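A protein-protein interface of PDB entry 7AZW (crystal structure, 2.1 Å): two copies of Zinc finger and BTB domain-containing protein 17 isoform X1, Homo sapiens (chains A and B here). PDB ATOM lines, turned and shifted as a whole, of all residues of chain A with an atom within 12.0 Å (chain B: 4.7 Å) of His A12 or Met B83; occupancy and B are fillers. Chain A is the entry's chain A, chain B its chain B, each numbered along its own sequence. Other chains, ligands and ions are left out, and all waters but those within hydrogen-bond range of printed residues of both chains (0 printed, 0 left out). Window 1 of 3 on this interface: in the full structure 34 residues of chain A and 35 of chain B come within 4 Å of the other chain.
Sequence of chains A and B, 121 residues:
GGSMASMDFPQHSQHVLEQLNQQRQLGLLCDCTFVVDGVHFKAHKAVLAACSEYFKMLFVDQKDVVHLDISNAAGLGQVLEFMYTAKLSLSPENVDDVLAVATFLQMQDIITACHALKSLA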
ATOM      1  N   MET A   7       7.732 -25.479   4.762  1.00  0.00           N
ATOM      2  CA  MET A   7       7.625 -24.080   5.149  1.00  0.00           C
ATOM      3  C   MET A   7       6.911 -23.935   6.487  1.00  0.00           C
ATOM      4  O   MET A   7       5.996 -24.695   6.813  1.00  0.00           O
ATOM      5  CB  MET A   7       6.884 -23.278   4.078  1.00  0.00           C
ATOM      6  CG  MET A   7       7.413 -23.495   2.669  1.00  0.00           C
ATOM      7  SD  MET A   7       6.840 -22.231   1.522  1.00  0.00           S
ATOM      8  CE  MET A   7       7.583 -20.765   2.234  1.00  0.00           C
ATOM      9  N   ASP A   8       7.342 -22.940   7.260  1.00  0.00           N
ATOM     10  CA  ASP A   8       6.729 -22.609   8.538  1.00  0.00           C
ATOM     11  C   ASP A   8       6.456 -21.114   8.583  1.00  0.00           C
ATOM     12  O   ASP A   8       7.330 -20.309   8.246  1.00  0.00           O
ATOM     13  CB  ASP A   8       7.623 -23.022   9.714  1.00  0.00           C
ATOM     14  CG  ASP A   8       6.989 -22.729  11.062  1.00  0.00           C
ATOM     15  OD1 ASP A   8       5.983 -23.389  11.405  1.00  0.00           O
ATOM     16  OD2 ASP A   8       7.494 -21.843  11.781  1.00  0.00           O
ATOM     17  N   PHE A   9       5.242 -20.748   9.000  1.00  0.00           N
ATOM     18  CA  PHE A   9       4.799 -19.359   9.077  1.00  0.00           C
ATOM     19  C   PHE A   9       4.654 -18.986  10.551  1.00  0.00           C
ATOM     20  O   PHE A   9       3.596 -19.204  11.152  1.00  0.00           O
ATOM     21  CB  PHE A   9       3.472 -19.171   8.333  1.00  0.00           C
ATOM     22  CG  PHE A   9       3.558 -19.437   6.850  1.00  0.00           C
ATOM     23  CD1 PHE A   9       3.717 -20.728   6.367  1.00  0.00           C
ATOM     24  CD2 PHE A   9       3.454 -18.399   5.941  1.00  0.00           C
ATOM     25  CE1 PHE A   9       3.793 -20.973   5.008  1.00  0.00           C
ATOM     26  CE2 PHE A   9       3.526 -18.639   4.579  1.00  0.00           C
ATOM     27  CZ  PHE A   9       3.696 -19.928   4.114  1.00  0.00           C
ATOM     28  N   PRO A  10       5.694 -18.417  11.173  1.00  0.00           N
ATOM     29  CA  PRO A  10       5.657 -18.232  12.636  1.00  0.00           C
ATOM     30  C   PRO A  10       4.645 -17.205  13.112  1.00  0.00           C
ATOM     31  O   PRO A  10       4.285 -17.226  14.296  1.00  0.00           O
ATOM     32  CB  PRO A  10       7.091 -17.794  12.966  1.00  0.00           C
ATOM     33  CG  PRO A  10       7.587 -17.165  11.707  1.00  0.00           C
ATOM     34  CD  PRO A  10       6.952 -17.935  10.583  1.00  0.00           C
ATOM     35  N   GLN A  11       4.172 -16.311  12.245  1.00  0.00           N
ATOM     36  CA  GLN A  11       3.221 -15.278  12.633  1.00  0.00           C
ATOM     37  C   GLN A  11       1.788 -15.618  12.241  1.00  0.00           C
ATOM     38  O   GLN A  11       0.905 -14.766  12.370  1.00  0.00           O
ATOM     39  CB  GLN A  11       3.619 -13.933  12.018  1.00  0.00           C
ATOM     40  CG  GLN A  11       5.119 -13.703  11.924  1.00  0.00           C
ATOM     41  CD  GLN A  11       5.800 -13.717  13.278  1.00  0.00           C
ATOM     42  OE1 GLN A  11       6.894 -14.261  13.428  1.00  0.00           O
ATOM     43  NE2 GLN A  11       5.158 -13.113  14.272  1.00  0.00           N
ATOM     44  N   HIS A  12       1.538 -16.842  11.771  1.00  0.00           N
ATOM     45  CA  HIS A  12       0.215 -17.181  11.259  1.00  0.00           C
ATOM     46  C   HIS A  12      -0.802 -17.368  12.380  1.00  0.00           C
ATOM     47  O   HIS A  12      -1.951 -16.932  12.250  1.00  0.00           O
ATOM     48  CB  HIS A  12       0.291 -18.439  10.395  1.00  0.00           C
ATOM     49  CG  HIS A  12      -1.048 -18.991  10.016  1.00  0.00           C
ATOM     50  ND1 HIS A  12      -1.538 -20.174  10.526  1.00  0.00           N
ATOM     51  CD2 HIS A  12      -2.004 -18.519   9.181  1.00  0.00           C
ATOM     52  CE1 HIS A  12      -2.734 -20.409  10.020  1.00  0.00           C
ATOM     53  NE2 HIS A  12      -3.042 -19.419   9.200  1.00  0.00           N
ATOM     54  N   SER A  13      -0.408 -18.019  13.479  1.00  0.00           N
ATOM     55  CA  SER A  13      -1.332 -18.202  14.594  1.00  0.00           C
ATOM     56  C   SER A  13      -1.736 -16.862  15.195  1.00  0.00           C
ATOM     57  O   SER A  13      -2.888 -16.677  15.605  1.00  0.00           O
ATOM     58  CB  SER A  13      -0.703 -19.100  15.658  1.00  0.00           C
ATOM     59  OG  SER A  13       0.358 -18.438  16.324  1.00  0.00           O
ATOM     60  N   GLN A  14      -0.798 -15.913  15.255  1.00  0.00           N
ATOM     61  CA  GLN A  14      -1.129 -14.572  15.718  1.00  0.00           C
ATOM     62  C   GLN A  14      -2.117 -13.896  14.776  1.00  0.00           C
ATOM     63  O   GLN A  14      -3.065 -13.240  15.223  1.00  0.00           O
ATOM     64  CB  GLN A  14       0.144 -13.738  15.848  1.00  0.00           C
ATOM     65  CG  GLN A  14       1.178 -14.329  16.790  1.00  0.00           C
ATOM     66  CD  GLN A  14       2.457 -13.519  16.830  1.00  0.00           C
ATOM     67  OE1 GLN A  14       3.555 -14.073  16.890  1.00  0.00           O
ATOM     68  NE2 GLN A  14       2.323 -12.197  16.798  1.00  0.00           N
ATOM     69  N   HIS A  15      -1.915 -14.053  13.466  1.00  0.00           N
ATOM     70  CA  HIS A  15      -2.817 -13.444  12.496  1.00  0.00           C
ATOM     71  C   HIS A  15      -4.209 -14.060  12.568  1.00  0.00           C
ATOM     72  O   HIS A  15      -5.213 -13.356  12.400  1.00  0.00           O
ATOM     73  CB  HIS A  15      -2.242 -13.583  11.086  1.00  0.00           C
ATOM     74  CG  HIS A  15      -3.137 -13.047  10.012  1.00  0.00           C
ATOM     75  ND1 HIS A  15      -3.865 -13.865   9.174  1.00  0.00           N
ATOM     76  CD2 HIS A  15      -3.421 -11.779   9.638  1.00  0.00           C
ATOM     77  CE1 HIS A  15      -4.559 -13.122   8.332  1.00  0.00           C
ATOM     78  NE2 HIS A  15      -4.307 -11.852   8.592  1.00  0.00           N
ATOM     79  N   VAL A  16      -4.291 -15.369  12.817  1.00  0.00           N
ATOM     80  CA  VAL A  16      -5.590 -16.032  12.907  1.00  0.00           C
ATOM     81  C   VAL A  16      -6.385 -15.487  14.089  1.00  0.00           C
ATOM     82  O   VAL A  16      -7.572 -15.166  13.966  1.00  0.00           O
ATOM     83  CB  VAL A  16      -5.410 -17.558  13.004  1.00  0.00           C
ATOM     84  CG1 VAL A  16      -6.719 -18.225  13.401  1.00  0.00           C
ATOM     85  CG2 VAL A  16      -4.902 -18.119  11.682  1.00  0.00           C
ATOM     86  N   LEU A  17      -5.736 -15.373  15.250  1.00  0.00           N
ATOM     87  CA  LEU A  17      -6.437 -14.897  16.438  1.00  0.00           C
ATOM     88  C   LEU A  17      -6.867 -13.442  16.285  1.00  0.00           C
ATOM     89  O   LEU A  17      -7.963 -13.067  16.717  1.00  0.00           O
ATOM     90  CB  LEU A  17      -5.555 -15.070  17.673  1.00  0.00           C
ATOM     91  CG  LEU A  17      -6.280 -14.896  19.009  1.00  0.00           C
ATOM     92  CD1 LEU A  17      -7.473 -15.835  19.085  1.00  0.00           C
ATOM     93  CD2 LEU A  17      -5.337 -15.138  20.173  1.00  0.00           C
ATOM     94  N   GLU A  18      -6.018 -12.609  15.678  1.00  0.00           N
ATOM     95  CA  GLU A  18      -6.398 -11.221  15.436  1.00  0.00           C
ATOM     96  C   GLU A  18      -7.596 -11.135  14.498  1.00  0.00           C
ATOM     97  O   GLU A  18      -8.480 -10.293  14.685  1.00  0.00           O
ATOM     98  CB  GLU A  18      -5.213 -10.441  14.867  1.00  0.00           C
ATOM     99  CG  GLU A  18      -4.057 -10.271  15.839  1.00  0.00           C
ATOM    100  CD  GLU A  18      -2.775  -9.850  15.149  1.00  0.00           C
ATOM    101  OE1 GLU A  18      -1.821  -9.453  15.851  1.00  0.00           O
ATOM    102  OE2 GLU A  18      -2.722  -9.912  13.902  1.00  0.00           O
ATOM    103  N   GLN A  19      -7.642 -12.002  13.484  1.00  0.00           N
ATOM    104  CA  GLN A  19      -8.798 -12.033  12.595  1.00  0.00           C
ATOM    105  C   GLN A  19     -10.041 -12.520  13.328  1.00  0.00           C
ATOM    106  O   GLN A  19     -11.145 -12.017  13.089  1.00  0.00           O
ATOM    107  CB  GLN A  19      -8.506 -12.918  11.384  1.00  0.00           C
ATOM    108  CG  GLN A  19      -7.523 -12.314  10.396  1.00  0.00           C
ATOM    109  CD  GLN A  19      -8.118 -11.154   9.625  1.00  0.00           C
ATOM    110  OE1 GLN A  19      -9.127 -11.304   8.935  1.00  0.00           O
ATOM    111  NE2 GLN A  19      -7.495  -9.986   9.739  1.00  0.00           N
ATOM    112  N   LEU A  20      -9.881 -13.496  14.226  1.00  0.00           N
ATOM    113  CA  LEU A  20     -11.015 -13.966  15.014  1.00  0.00           C
ATOM    114  C   LEU A  20     -11.508 -12.883  15.965  1.00  0.00           C
ATOM    115  O   LEU A  20     -12.715 -12.758  16.201  1.00  0.00           O
ATOM    116  CB  LEU A  20     -10.633 -15.228  15.786  1.00  0.00           C
ATOM    117  CG  LEU A  20     -10.403 -16.486  14.946  1.00  0.00           C
ATOM    118  CD1 LEU A  20      -9.805 -17.599  15.793  1.00  0.00           C
ATOM    119  CD2 LEU A  20     -11.700 -16.940  14.298  1.00  0.00           C
ATOM    120  N   ASN A  21     -10.589 -12.090  16.522  1.00  0.00           N
ATOM    121  CA  ASN A  21     -10.995 -10.969  17.361  1.00  0.00           C
ATOM    122  C   ASN A  21     -11.687  -9.886  16.544  1.00  0.00           C
ATOM    123  O   ASN A  21     -12.570  -9.192  17.059  1.00  0.00           O
ATOM    124  CB  ASN A  21      -9.785 -10.391  18.094  1.00  0.00           C
ATOM    125  CG  ASN A  21     -10.180  -9.460  19.225  1.00  0.00           C
ATOM    126  OD1 ASN A  21     -11.143  -9.716  19.948  1.00  0.00           O
ATOM    127  ND2 ASN A  21      -9.436  -8.371  19.381  1.00  0.00           N
ATOM    128  N   GLN A  23     -13.557 -10.551  13.831  1.00  0.00           N
ATOM    129  CA  GLN A  23     -14.893 -11.104  13.637  1.00  0.00           C
ATOM    130  C   GLN A  23     -15.769 -10.858  14.858  1.00  0.00           C
ATOM    131  O   GLN A  23     -16.956 -10.537  14.727  1.00  0.00           O
ATOM    132  CB  GLN A  23     -14.811 -12.604  13.345  1.00  0.00           C
ATOM    133  CG  GLN A  23     -14.045 -12.976  12.090  1.00  0.00           C
ATOM    134  CD  GLN A  23     -13.876 -14.476  11.950  1.00  0.00           C
ATOM    135  OE1 GLN A  23     -14.490 -15.253  12.684  1.00  0.00           O
ATOM    136  NE2 GLN A  23     -13.040 -14.894  11.006  1.00  0.00           N
ATOM    137  N   LEU A  29     -19.959 -14.313  12.433  1.00  0.00           N
ATOM    138  CA  LEU A  29     -19.656 -15.731  12.620  1.00  0.00           C
ATOM    139  C   LEU A  29     -19.564 -16.127  14.090  1.00  0.00           C
ATOM    140  O   LEU A  29     -18.997 -17.174  14.420  1.00  0.00           O
ATOM    141  CB  LEU A  29     -18.371 -16.125  11.883  1.00  0.00           C
ATOM    142  CG  LEU A  29     -18.317 -15.742  10.403  1.00  0.00           C
ATOM    143  CD1 LEU A  29     -17.015 -16.208   9.772  1.00  0.00           C
ATOM    144  CD2 LEU A  29     -19.512 -16.308   9.648  1.00  0.00           C
ATOM    145  N   ALA A  46     -15.875 -22.287  19.414  1.00  0.00           N
ATOM    146  CA  ALA A  46     -14.613 -22.993  19.219  1.00  0.00           C
ATOM    147  C   ALA A  46     -13.460 -22.282  19.914  1.00  0.00           C
ATOM    148  O   ALA A  46     -12.560 -22.934  20.457  1.00  0.00           O
ATOM    149  CB  ALA A  46     -14.325 -23.148  17.727  1.00  0.00           C
ATOM    150  N   VAL A  47     -13.466 -20.948  19.908  1.00  0.00           N
ATOM    151  CA  VAL A  47     -12.388 -20.200  20.549  1.00  0.00           C
ATOM    152  C   VAL A  47     -12.456 -20.361  22.063  1.00  0.00           C
ATOM    153  O   VAL A  47     -11.439 -20.606  22.722  1.00  0.00           O
ATOM    154  CB  VAL A  47     -12.438 -18.718  20.133  1.00  0.00           C
ATOM    155  CG1 VAL A  47     -11.418 -17.914  20.923  1.00  0.00           C
ATOM    156  CG2 VAL A  47     -12.190 -18.575  18.638  1.00  0.00           C
ATOM    157  N   ALA A  50     -11.334 -23.630  22.950  1.00  0.00           N
ATOM    158  CA  ALA A  50      -9.901 -23.794  22.732  1.00  0.00           C
ATOM    159  C   ALA A  50      -9.084 -23.320  23.927  1.00  0.00           C
ATOM    160  O   ALA A  50      -7.980 -23.826  24.159  1.00  0.00           O
ATOM    161  CB  ALA A  50      -9.472 -23.046  21.469  1.00  0.00           C
ATOM    162  N   TYR A  84      -9.027 -13.694  23.326  1.00  0.00           N
ATOM    163  CA  TYR A  84      -8.935 -13.163  21.974  1.00  0.00           C
ATOM    164  C   TYR A  84      -7.712 -12.287  21.746  1.00  0.00           C
ATOM    165  O   TYR A  84      -7.287 -12.140  20.595  1.00  0.00           O
ATOM    166  CB  TYR A  84     -10.199 -12.364  21.632  1.00  0.00           C
ATOM    167  CG  TYR A  84     -11.372 -13.231  21.229  1.00  0.00           C
ATOM    168  CD1 TYR A  84     -11.573 -13.583  19.902  1.00  0.00           C
ATOM    169  CD2 TYR A  84     -12.275 -13.698  22.176  1.00  0.00           C
ATOM    170  CE1 TYR A  84     -12.641 -14.377  19.526  1.00  0.00           C
ATOM    171  CE2 TYR A  84     -13.349 -14.493  21.808  1.00  0.00           C
ATOM    172  CZ  TYR A  84     -13.526 -14.829  20.481  1.00  0.00           C
ATOM    173  OH  TYR A  84     -14.589 -15.618  20.105  1.00  0.00           O
ATOM    174  N   LEU B  17      -4.510 -22.067  18.372  1.00  0.00           N
ATOM    175  CA  LEU B  17      -4.528 -22.727  17.071  1.00  0.00           C
ATOM    176  C   LEU B  17      -4.319 -24.230  17.208  1.00  0.00           C
ATOM    177  O   LEU B  17      -4.960 -25.016  16.502  1.00  0.00           O
ATOM    178  CB  LEU B  17      -3.466 -22.120  16.158  1.00  0.00           C
ATOM    179  CG  LEU B  17      -3.563 -22.522  14.685  1.00  0.00           C
ATOM    180  CD1 LEU B  17      -4.871 -22.025  14.085  1.00  0.00           C
ATOM    181  CD2 LEU B  17      -2.368 -22.000  13.901  1.00  0.00           C
ATOM    182  N   VAL B  47     -12.447 -20.147  11.373  1.00  0.00           N
ATOM    183  CA  VAL B  47     -11.035 -20.332  11.047  1.00  0.00           C
ATOM    184  C   VAL B  47     -10.808 -20.157   9.551  1.00  0.00           C
ATOM    185  O   VAL B  47      -9.812 -19.558   9.126  1.00  0.00           O
ATOM    186  CB  VAL B  47     -10.549 -21.709  11.535  1.00  0.00           C
ATOM    187  CG1 VAL B  47      -9.085 -21.917  11.174  1.00  0.00           C
ATOM    188  CG2 VAL B  47     -10.754 -21.847  13.037  1.00  0.00           C
ATOM    189  N   LEU B  48     -11.723 -20.678   8.732  1.00  0.00           N
ATOM    190  CA  LEU B  48     -11.597 -20.538   7.284  1.00  0.00           C
ATOM    191  C   LEU B  48     -11.648 -19.076   6.870  1.00  0.00           C
ATOM    192  O   LEU B  48     -10.846 -18.622   6.046  1.00  0.00           O
ATOM    193  CB  LEU B  48     -12.706 -21.324   6.585  1.00  0.00           C
ATOM    194  CG  LEU B  48     -12.427 -22.775   6.198  1.00  0.00           C
ATOM    195  CD1 LEU B  48     -11.956 -23.579   7.386  1.00  0.00           C
ATOM    196  CD2 LEU B  48     -13.686 -23.378   5.634  1.00  0.00           C
ATOM    197  N   CYS B  51      -8.474 -17.034   7.352  1.00  0.00           N
ATOM    198  CA  CYS B  51      -7.306 -17.380   6.555  1.00  0.00           C
ATOM    199  C   CYS B  51      -7.517 -17.251   5.051  1.00  0.00           C
ATOM    200  O   CYS B  51      -6.534 -17.129   4.314  1.00  0.00           O
ATOM    201  CB  CYS B  51      -6.866 -18.817   6.856  1.00  0.00           C
ATOM    202  SG  CYS B  51      -6.236 -19.116   8.524  1.00  0.00           S
ATOM    203  N   VAL B  79      -3.648 -27.254   2.267  1.00  0.00           N
ATOM    204  CA  VAL B  79      -4.022 -25.874   2.563  1.00  0.00           C
ATOM    205  C   VAL B  79      -4.749 -25.798   3.900  1.00  0.00           C
ATOM    206  O   VAL B  79      -4.460 -24.933   4.736  1.00  0.00           O
ATOM    207  CB  VAL B  79      -4.877 -25.293   1.423  1.00  0.00           C
ATOM    208  CG1 VAL B  79      -5.490 -23.969   1.841  1.00  0.00           C
ATOM    209  CG2 VAL B  79      -4.039 -25.122   0.168  1.00  0.00           C
ATOM    210  N   LEU B  80      -5.703 -26.706   4.121  1.00  0.00           N
ATOM    211  CA  LEU B  80      -6.403 -26.761   5.399  1.00  0.00           C
ATOM    212  C   LEU B  80      -5.450 -27.091   6.543  1.00  0.00           C
ATOM    213  O   LEU B  80      -5.659 -26.639   7.675  1.00  0.00           O
ATOM    214  CB  LEU B  80      -7.533 -27.792   5.330  1.00  0.00           C
ATOM    215  CG  LEU B  80      -8.783 -27.466   4.500  1.00  0.00           C
ATOM    216  CD1 LEU B  80      -9.704 -28.672   4.434  1.00  0.00           C
ATOM    217  CD2 LEU B  80      -9.541 -26.247   5.049  1.00  0.00           C
ATOM    218  N   GLU B  81      -4.408 -27.884   6.271  1.00  0.00           N
ATOM    219  CA  GLU B  81      -3.395 -28.160   7.285  1.00  0.00           C
ATOM    220  C   GLU B  81      -2.601 -26.906   7.630  1.00  0.00           C
ATOM    221  O   GLU B  81      -2.290 -26.662   8.802  1.00  0.00           O
ATOM    222  CB  GLU B  81      -2.459 -29.269   6.801  1.00  0.00           C
ATOM    223  CG  GLU B  81      -1.393 -29.679   7.802  1.00  0.00           C
ATOM    224  CD  GLU B  81      -1.914 -30.643   8.850  1.00  0.00           C
ATOM    225  OE1 GLU B  81      -1.146 -30.996   9.770  1.00  0.00           O
ATOM    226  OE2 GLU B  81      -3.092 -31.049   8.754  1.00  0.00           O
ATOM    227  N   PHE B  82      -2.258 -26.103   6.620  1.00  0.00           N
ATOM    228  CA  PHE B  82      -1.555 -24.850   6.877  1.00  0.00           C
ATOM    229  C   PHE B  82      -2.403 -23.907   7.720  1.00  0.00           C
ATOM    230  O   PHE B  82      -1.879 -23.181   8.572  1.00  0.00           O
ATOM    231  CB  PHE B  82      -1.168 -24.182   5.558  1.00  0.00           C
ATOM    232  CG  PHE B  82      -1.044 -22.683   5.647  1.00  0.00           C
ATOM    233  CD1 PHE B  82       0.124 -22.098   6.110  1.00  0.00           C
ATOM    234  CD2 PHE B  82      -2.095 -21.860   5.270  1.00  0.00           C
ATOM    235  CE1 PHE B  82       0.240 -20.723   6.194  1.00  0.00           C
ATOM    236  CE2 PHE B  82      -1.984 -20.485   5.353  1.00  0.00           C
ATOM    237  CZ  PHE B  82      -0.814 -19.916   5.816  1.00  0.00           C
ATOM    238  N   MET B  83      -3.720 -23.906   7.498  1.00  0.00           N
ATOM    239  CA  MET B  83      -4.583 -22.966   8.204  1.00  0.00           C
ATOM    240  C   MET B  83      -4.670 -23.297   9.687  1.00  0.00           C
ATOM    241  O   MET B  83      -4.948 -22.411  10.503  1.00  0.00           O
ATOM    242  CB  MET B  83      -5.980 -22.974   7.590  1.00  0.00           C
ATOM    243  CG  MET B  83      -6.025 -22.562   6.126  1.00  0.00           C
ATOM    244  SD  MET B  83      -7.601 -21.813   5.670  1.00  0.00           S
ATOM    245  CE  MET B  83      -8.732 -23.096   6.137  1.00  0.00           C
ATOM    246  N   TYR B  84      -4.434 -24.559  10.052  1.00  0.00           N
ATOM    247  CA  TYR B  84      -4.539 -25.002  11.433  1.00  0.00           C
ATOM    248  C   TYR B  84      -3.195 -25.287  12.086  1.00  0.00           C
ATOM    249  O   TYR B  84      -3.156 -25.512  13.301  1.00  0.00           O
ATOM    250  CB  TYR B  84      -5.420 -26.260  11.522  1.00  0.00           C
ATOM    251  CG  TYR B  84      -6.904 -25.973  11.453  1.00  0.00           C
ATOM    252  CD1 TYR B  84      -7.550 -25.836  10.229  1.00  0.00           C
ATOM    253  CD2 TYR B  84      -7.659 -25.830  12.609  1.00  0.00           C
ATOM    254  CE1 TYR B  84      -8.907 -25.569  10.159  1.00  0.00           C
ATOM    255  CE2 TYR B  84      -9.016 -25.564  12.549  1.00  0.00           C
ATOM    256  CZ  TYR B  84      -9.635 -25.435  11.324  1.00  0.00           C
ATOM    257  OH  TYR B  84     -10.985 -25.168  11.269  1.00  0.00           O
ATOM    258  N   THR B  85      -2.097 -25.298  11.323  1.00  0.00           N
ATOM    259  CA  THR B  85      -0.780 -25.585  11.878  1.00  0.00           C
ATOM    260  C   THR B  85       0.296 -24.585  11.480  1.00  0.00           C
ATOM    261  O   THR B  85       1.403 -24.657  12.029  1.00  0.00           O
ATOM    262  CB  THR B  85      -0.307 -26.989  11.461  1.00  0.00           C
ATOM    263  OG1 THR B  85      -0.161 -27.043  10.036  1.00  0.00           O
ATOM    264  CG2 THR B  85      -1.302 -28.053  11.907  1.00  0.00           C
ATOM    265  N   ALA B  86       0.015 -23.668  10.550  1.00  0.00           N
ATOM    266  CA  ALA B  86       0.992 -22.698  10.050  1.00  0.00           C
ATOM    267  C   ALA B  86       2.179 -23.382   9.376  1.00  0.00           C
ATOM    268  O   ALA B  86       3.285 -22.836   9.337  1.00  0.00           O
ATOM    269  CB  ALA B  86       1.476 -21.761  11.161  1.00  0.00           C
ATOM    270  N   MET B 107      -5.766 -17.064  -1.285  1.00  0.00           N
ATOM    271  CA  MET B 107      -4.787 -16.993  -0.203  1.00  0.00           C
ATOM    272  C   MET B 107      -3.445 -16.600  -0.809  1.00  0.00           C
ATOM    273  O   MET B 107      -2.696 -17.451  -1.294  1.00  0.00           O
ATOM    274  CB  MET B 107      -4.709 -18.321   0.538  1.00  0.00           C
ATOM    275  CG  MET B 107      -6.051 -18.801   1.062  1.00  0.00           C
ATOM    276  SD  MET B 107      -5.976 -20.443   1.797  1.00  0.00           S
ATOM    277  CE  MET B 107      -4.876 -20.146   3.178  1.00  0.00           C
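The backbone carbonyl oxygen of Ala B86 lies within hydrogen-bond range of the backbone NH of Phe A9 (2.9 Å). NE2 of His A12 sits at hydrogen-bond distance from SG of Cys B51, 3.3 Å away. The backbone carbonyl oxygen (O) of Ala B86 lies close to the side-chain carboxylate (OD1) of Asp A8 (3.4 Å).
O of Val B47 sits at hydrogen-bond distance from SG of Cys B51 (3.7 Å).
Among the printed residues, pairs that only touch across the chains: Phe A9 with Phe B82 (3.5 Å), His A12 with Leu B17 (3.9 Å), His A12 with Phe B82 (3.2 Å), His A12 with Met B83 (3.0 Å), His A12 with Ala B86 (3.5 Å), Ser A13 with Leu B17 (3.8 Å) and Val A16 with Cys B51 (3.6 Å).
Of the printed residues of chain B, Phe A9 touches Phe B82 (3.5 Å) and Ala B86 (2.9 Å). Printed residues of chain B within 4 Å of Ser A13: Leu B17 (3.8 Å). Ala A50 touches none of the printed residues of chain B. No residue of chain A comes within 4 Å of Leu B48. Of the printed residues of chain A, Cys B51 touches His A12 (3.3 Å) and Val A16 (3.6 Å). No residue of chain A comes within 4 Å of Val B79. Of chain A, only His A12 (3.0 Å) comes within 4 Å of Met B83. No residue of chain A comes within 4 Å of Tyr B84. Ala B86 touches just these residues of chain A: Asp A8, Phe A9 and His A12. The nearest printed residue of chain B that does not touch Asp A8 is Thr B85 (4.8 Å).
Hydrophobic or aromatic side chains of chain A that line the printed part of chain B: Phe A9, His A12 and Val A16. Hydrophobic or aromatic side chains of chain B within 4 Å of the printed part of chain A: Leu B17, Phe B82 and Ala B86. Among the printed residues, 10 pairs touch across the chains. Among the printed residues, no Asp or Glu carboxylate lies within 4 Å of a Lys or Arg side-chain nitrogen of the other chain.
Positions printed for both chains: 17, 47 and 84. Of the 10 pairs that touch across the chains among the printed residues, none has its exchanged pair printed and touching as well.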
